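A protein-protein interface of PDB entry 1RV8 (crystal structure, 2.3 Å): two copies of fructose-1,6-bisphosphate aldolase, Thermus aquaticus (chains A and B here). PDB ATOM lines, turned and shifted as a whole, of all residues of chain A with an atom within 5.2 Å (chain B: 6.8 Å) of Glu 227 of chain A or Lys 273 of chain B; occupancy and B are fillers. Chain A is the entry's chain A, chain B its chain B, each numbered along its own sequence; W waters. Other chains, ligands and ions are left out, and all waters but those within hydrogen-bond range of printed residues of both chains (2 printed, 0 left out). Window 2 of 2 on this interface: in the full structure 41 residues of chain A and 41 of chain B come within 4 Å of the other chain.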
ATOM      1  N   PHE A 221      37.056 -25.996  12.663  1.00  0.00           N
ATOM      2  CA  PHE A 221      35.763 -25.408  12.993  1.00  0.00           C
ATOM      3  C   PHE A 221      34.702 -26.492  13.150  1.00  0.00           C
ATOM      4  O   PHE A 221      33.941 -26.495  14.120  1.00  0.00           O
ATOM      5  CB  PHE A 221      35.349 -24.419  11.895  1.00  0.00           C
ATOM      6  CG  PHE A 221      34.018 -23.761  12.130  1.00  0.00           C
ATOM      7  CD1 PHE A 221      33.765 -23.071  13.314  1.00  0.00           C
ATOM      8  CD2 PHE A 221      33.022 -23.814  11.156  1.00  0.00           C
ATOM      9  CE1 PHE A 221      32.541 -22.441  13.528  1.00  0.00           C
ATOM     10  CE2 PHE A 221      31.789 -23.186  11.358  1.00  0.00           C
ATOM     11  CZ  PHE A 221      31.548 -22.497  12.549  1.00  0.00           C
ATOM     12  N   ARG A 222      34.653 -27.410  12.187  1.00  0.00           N
ATOM     13  CA  ARG A 222      33.680 -28.499  12.216  1.00  0.00           C
ATOM     14  C   ARG A 222      33.904 -29.421  13.407  1.00  0.00           C
ATOM     15  O   ARG A 222      32.951 -29.894  14.023  1.00  0.00           O
ATOM     16  CB  ARG A 222      33.755 -29.332  10.932  1.00  0.00           C
ATOM     17  CG  ARG A 222      33.307 -28.620   9.662  1.00  0.00           C
ATOM     18  CD  ARG A 222      32.613 -29.613   8.732  1.00  0.00           C
ATOM     19  NE  ARG A 222      32.259 -29.043   7.434  1.00  0.00           N
ATOM     20  CZ  ARG A 222      33.088 -28.970   6.395  1.00  0.00           C
ATOM     21  NH1 ARG A 222      34.330 -29.431   6.496  1.00  0.00           N
ATOM     22  NH2 ARG A 222      32.671 -28.450   5.247  1.00  0.00           N
ATOM     23  N   GLY A 225      32.371 -28.475  16.489  1.00  0.00           N
ATOM     24  CA  GLY A 225      30.920 -28.513  16.437  1.00  0.00           C
ATOM     25  C   GLY A 225      30.341 -27.593  15.377  1.00  0.00           C
ATOM     26  O   GLY A 225      29.155 -27.652  15.063  1.00  0.00           O
ATOM     27  N   GLY A 226      31.181 -26.734  14.820  1.00  0.00           N
ATOM     28  CA  GLY A 226      30.701 -25.815  13.809  1.00  0.00           C
ATOM     29  C   GLY A 226      30.184 -26.538  12.585  1.00  0.00           C
ATOM     30  O   GLY A 226      30.613 -27.652  12.283  1.00  0.00           O
ATOM     31  N   GLU A 227      29.249 -25.912  11.882  1.00  0.00           N
ATOM     32  CA  GLU A 227      28.702 -26.507  10.673  1.00  0.00           C
ATOM     33  C   GLU A 227      28.837 -25.513   9.539  1.00  0.00           C
ATOM     34  O   GLU A 227      28.377 -24.375   9.632  1.00  0.00           O
ATOM     35  CB  GLU A 227      27.240 -26.893  10.874  1.00  0.00           C
ATOM     36  CG  GLU A 227      27.011 -27.707  12.135  1.00  0.00           C
ATOM     37  CD  GLU A 227      25.667 -28.406  12.150  1.00  0.00           C
ATOM     38  OE1 GLU A 227      24.666 -27.800  11.704  1.00  0.00           O
ATOM     39  OE2 GLU A 227      25.617 -29.560  12.622  1.00  0.00           O
ATOM     40  N   ILE A 228      29.486 -25.953   8.468  1.00  0.00           N
ATOM     41  CA  ILE A 228      29.713 -25.111   7.308  1.00  0.00           C
ATOM     42  C   ILE A 228      29.768 -25.980   6.049  1.00  0.00           C
ATOM     43  O   ILE A 228      30.177 -27.145   6.102  1.00  0.00           O
ATOM     44  CB  ILE A 228      31.034 -24.333   7.481  1.00  0.00           C
ATOM     45  CG1 ILE A 228      31.204 -23.318   6.357  1.00  0.00           C
ATOM     46  CG2 ILE A 228      32.206 -25.304   7.520  1.00  0.00           C
ATOM     47  CD1 ILE A 228      32.397 -22.409   6.556  1.00  0.00           C
ATOM     48  N   GLY A 229      29.341 -25.410   4.927  1.00  0.00           N
ATOM     49  CA  GLY A 229      29.338 -26.137   3.671  1.00  0.00           C
ATOM     50  C   GLY A 229      30.720 -26.271   3.059  1.00  0.00           C
ATOM     51  O   GLY A 229      31.731 -26.167   3.762  1.00  0.00           O
ATOM     52  N   ARG A 265      34.578 -22.373  20.857  1.00  0.00           N
ATOM     53  CA  ARG A 265      33.858 -23.638  20.902  1.00  0.00           C
ATOM     54  C   ARG A 265      34.633 -24.757  21.585  1.00  0.00           C
ATOM     55  O   ARG A 265      34.075 -25.479  22.413  1.00  0.00           O
ATOM     56  CB  ARG A 265      33.481 -24.080  19.495  1.00  0.00           C
ATOM     57  CG  ARG A 265      32.262 -23.386  18.963  1.00  0.00           C
ATOM     58  CD  ARG A 265      31.936 -23.890  17.577  1.00  0.00           C
ATOM     59  NE  ARG A 265      30.546 -23.623  17.241  1.00  0.00           N
ATOM     60  CZ  ARG A 265      29.525 -24.348  17.677  1.00  0.00           C
ATOM     61  NH1 ARG A 265      29.739 -25.394  18.461  1.00  0.00           N
ATOM     62  NH2 ARG A 265      28.291 -24.016  17.336  1.00  0.00           N
ATOM     63  N   LEU B 268      25.726 -20.718  20.753  1.00  0.00           N
ATOM     64  CA  LEU B 268      26.563 -21.663  20.032  1.00  0.00           C
ATOM     65  C   LEU B 268      25.935 -23.056  19.963  1.00  0.00           C
ATOM     66  O   LEU B 268      26.142 -23.784  18.992  1.00  0.00           O
ATOM     67  CB  LEU B 268      27.961 -21.727  20.657  1.00  0.00           C
ATOM     68  CG  LEU B 268      28.811 -20.461  20.488  1.00  0.00           C
ATOM     69  CD1 LEU B 268      30.175 -20.665  21.135  1.00  0.00           C
ATOM     70  CD2 LEU B 268      28.975 -20.144  19.010  1.00  0.00           C
ATOM     71  N   LYS B 270      22.702 -23.657  19.844  1.00  0.00           N
ATOM     72  CA  LYS B 270      21.582 -23.541  18.923  1.00  0.00           C
ATOM     73  C   LYS B 270      21.938 -23.167  17.486  1.00  0.00           C
ATOM     74  O   LYS B 270      21.232 -23.550  16.553  1.00  0.00           O
ATOM     75  CB  LYS B 270      20.580 -22.527  19.482  1.00  0.00           C
ATOM     76  CG  LYS B 270      19.369 -22.259  18.598  1.00  0.00           C
ATOM     77  CD  LYS B 270      18.438 -21.251  19.262  1.00  0.00           C
ATOM     78  CE  LYS B 270      17.253 -20.895  18.370  1.00  0.00           C
ATOM     79  NZ  LYS B 270      16.339 -19.892  19.010  1.00  0.00           N
ATOM     80  N   ASN B 271      23.025 -22.425  17.303  1.00  0.00           N
ATOM     81  CA  ASN B 271      23.416 -21.990  15.967  1.00  0.00           C
ATOM     82  C   ASN B 271      24.833 -22.411  15.598  1.00  0.00           C
ATOM     83  O   ASN B 271      25.720 -21.572  15.465  1.00  0.00           O
ATOM     84  CB  ASN B 271      23.302 -20.472  15.884  1.00  0.00           C
ATOM     85  CG  ASN B 271      21.946 -19.968  16.327  1.00  0.00           C
ATOM     86  OD1 ASN B 271      21.009 -19.899  15.537  1.00  0.00           O
ATOM     87  ND2 ASN B 271      21.834 -19.622  17.603  1.00  0.00           N
ATOM     88  N   PRO B 272      25.060 -23.718  15.406  1.00  0.00           N
ATOM     89  CA  PRO B 272      26.389 -24.222  15.053  1.00  0.00           C
ATOM     90  C   PRO B 272      26.966 -23.652  13.758  1.00  0.00           C
ATOM     91  O   PRO B 272      28.172 -23.738  13.524  1.00  0.00           O
ATOM     92  CB  PRO B 272      26.168 -25.732  14.983  1.00  0.00           C
ATOM     93  CG  PRO B 272      24.749 -25.833  14.515  1.00  0.00           C
ATOM     94  CD  PRO B 272      24.068 -24.808  15.385  1.00  0.00           C
ATOM     95  N   LYS B 273      26.112 -23.075  12.919  1.00  0.00           N
ATOM     96  CA  LYS B 273      26.561 -22.497  11.649  1.00  0.00           C
ATOM     97  C   LYS B 273      27.052 -21.061  11.832  1.00  0.00           C
ATOM     98  O   LYS B 273      27.537 -20.433  10.891  1.00  0.00           O
ATOM     99  CB  LYS B 273      25.414 -22.502  10.631  1.00  0.00           C
ATOM    100  CG  LYS B 273      24.996 -23.889  10.170  1.00  0.00           C
ATOM    101  CD  LYS B 273      23.626 -23.880   9.481  1.00  0.00           C
ATOM    102  CE  LYS B 273      23.636 -23.119   8.163  1.00  0.00           C
ATOM    103  NZ  LYS B 273      22.266 -23.064   7.553  1.00  0.00           N
ATOM    104  N   GLU B 274      26.936 -20.558  13.054  1.00  0.00           N
ATOM    105  CA  GLU B 274      27.322 -19.188  13.374  1.00  0.00           C
ATOM    106  C   GLU B 274      28.796 -18.974  13.719  1.00  0.00           C
ATOM    107  O   GLU B 274      29.332 -19.611  14.627  1.00  0.00           O
ATOM    108  CB  GLU B 274      26.472 -18.705  14.543  1.00  0.00           C
ATOM    109  CG  GLU B 274      26.545 -17.224  14.809  1.00  0.00           C
ATOM    110  CD  GLU B 274      25.949 -16.427  13.685  1.00  0.00           C
ATOM    111  OE1 GLU B 274      26.708 -15.976  12.804  1.00  0.00           O
ATOM    112  OE2 GLU B 274      24.711 -16.268  13.673  1.00  0.00           O
ATOM    113  N   PHE B 275      29.457 -18.083  12.990  1.00  0.00           N
ATOM    114  CA  PHE B 275      30.840 -17.773  13.301  1.00  0.00           C
ATOM    115  C   PHE B 275      31.086 -16.261  13.302  1.00  0.00           C
ATOM    116  O   PHE B 275      32.226 -15.806  13.285  1.00  0.00           O
ATOM    117  CB  PHE B 275      31.815 -18.527  12.382  1.00  0.00           C
ATOM    118  CG  PHE B 275      31.661 -18.232  10.919  1.00  0.00           C
ATOM    119  CD1 PHE B 275      32.153 -17.051  10.373  1.00  0.00           C
ATOM    120  CD2 PHE B 275      31.072 -19.167  10.069  1.00  0.00           C
ATOM    121  CE1 PHE B 275      32.065 -16.810   9.003  1.00  0.00           C
ATOM    122  CE2 PHE B 275      30.981 -18.933   8.701  1.00  0.00           C
ATOM    123  CZ  PHE B 275      31.479 -17.757   8.169  1.00  0.00           C
ATOM    124  N   ASP B 276      29.997 -15.494  13.332  1.00  0.00           N
ATOM    125  CA  ASP B 276      30.064 -14.035  13.411  1.00  0.00           C
ATOM    126  C   ASP B 276      30.022 -13.739  14.910  1.00  0.00           C
ATOM    127  O   ASP B 276      28.981 -13.873  15.548  1.00  0.00           O
ATOM    128  CB  ASP B 276      28.851 -13.387  12.737  1.00  0.00           C
ATOM    129  CG  ASP B 276      28.836 -11.867  12.884  1.00  0.00           C
ATOM    130  OD1 ASP B 276      29.626 -11.332  13.691  1.00  0.00           O
ATOM    131  OD2 ASP B 276      28.025 -11.203  12.200  1.00  0.00           O
HETATM  132  O   HOH W   1      26.102 -26.544  18.354  1.00  0.00           O
HETATM  133  O   HOH W   2      29.400 -22.192  15.442  1.00  0.00           O
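No position is printed for both chains. Of the 8 pairs that touch across the chains among the printed residues, none has its exchanged pair printed and touching as well.
The backbone NH (N) of Glu 227 of chain A sits at hydrogen-bond distance from the backbone carbonyl oxygen (O) of Pro 272 of chain B, 2.9 Å away. The guanidinium group of Arg 265 of chain A lies within hydrogen-bond range of the backbone carbonyl oxygen of Leu 268 of chain B (2.7 Å).
The backbone carbonyl oxygen (O) of Phe 221 of chain A sits at hydrogen-bond distance from the backbone NH (N) of Gly 226 of chain A (2.9 Å).
Water W2 lies within hydrogen-bond range of NE of Arg 265 of chain A (2.6 Å), O of Glu 274 of chain B (2.7 Å) and O of Pro 272 of chain B (2.8 Å). Water W1 bridges O of Leu 268 of chain B (2.8 Å) and NH2 of Arg 265 of chain A (3.5 Å).
Lys 273 of chain B touches one residue of chain A. Of the printed residues of chain B, Gly 225 of chain A touches Pro 272. Of the printed residues of chain B, Phe 221 of chain A touches Pro 272 (3.7 Å) and Phe 275 (3.98 Å). Of the printed residues of chain A, Phe 275 of chain B touches Phe 221. Of the printed residues of chain B, Arg 265 of chain A touches Leu 268 and Pro 272. Printed residues of chain B within 4 Å of Gly 226 of chain A: Pro 272 (3.3 Å). Asp 276 of chain B touches none of the printed residues of chain A. The nearest residue of chain B that does not touch Glu 227 of chain A is Glu 274 of chain B (5.3 Å). The nearest residue of chain A that does not touch Lys 273 of chain B is Phe 221 of chain A (4.8 Å). The nearest printed residue of chain A that does not touch Leu 268 of chain B is Gly 225 of chain A (6.3 Å).
Among the printed residues, merely in contact across the chains: Phe 221 of chain A with Pro 272 of chain B (3.7 Å), Phe 221 of chain A with Phe 275 of chain B (3.98 Å), Gly 225 of chain A with Pro 272 of chain B (3.6 Å), Gly 226 of chain A with Pro 272 of chain B (3.3 Å), Glu 227 of chain A with Lys 273 of chain B (3.3 Å) and Arg 265 of chain A with Pro 272 of chain B (3.0 Å).
Printed residues of chain B that touch a printed residue of chain A: Leu 268, Pro 272, Lys 273 and Phe 275. Among the printed residues, 8 pairs touch across the chains. Among the printed residues, no Asp or Glu carboxylate lies within 4 Å of a Lys or Arg side-chain nitrogen of the other chain.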
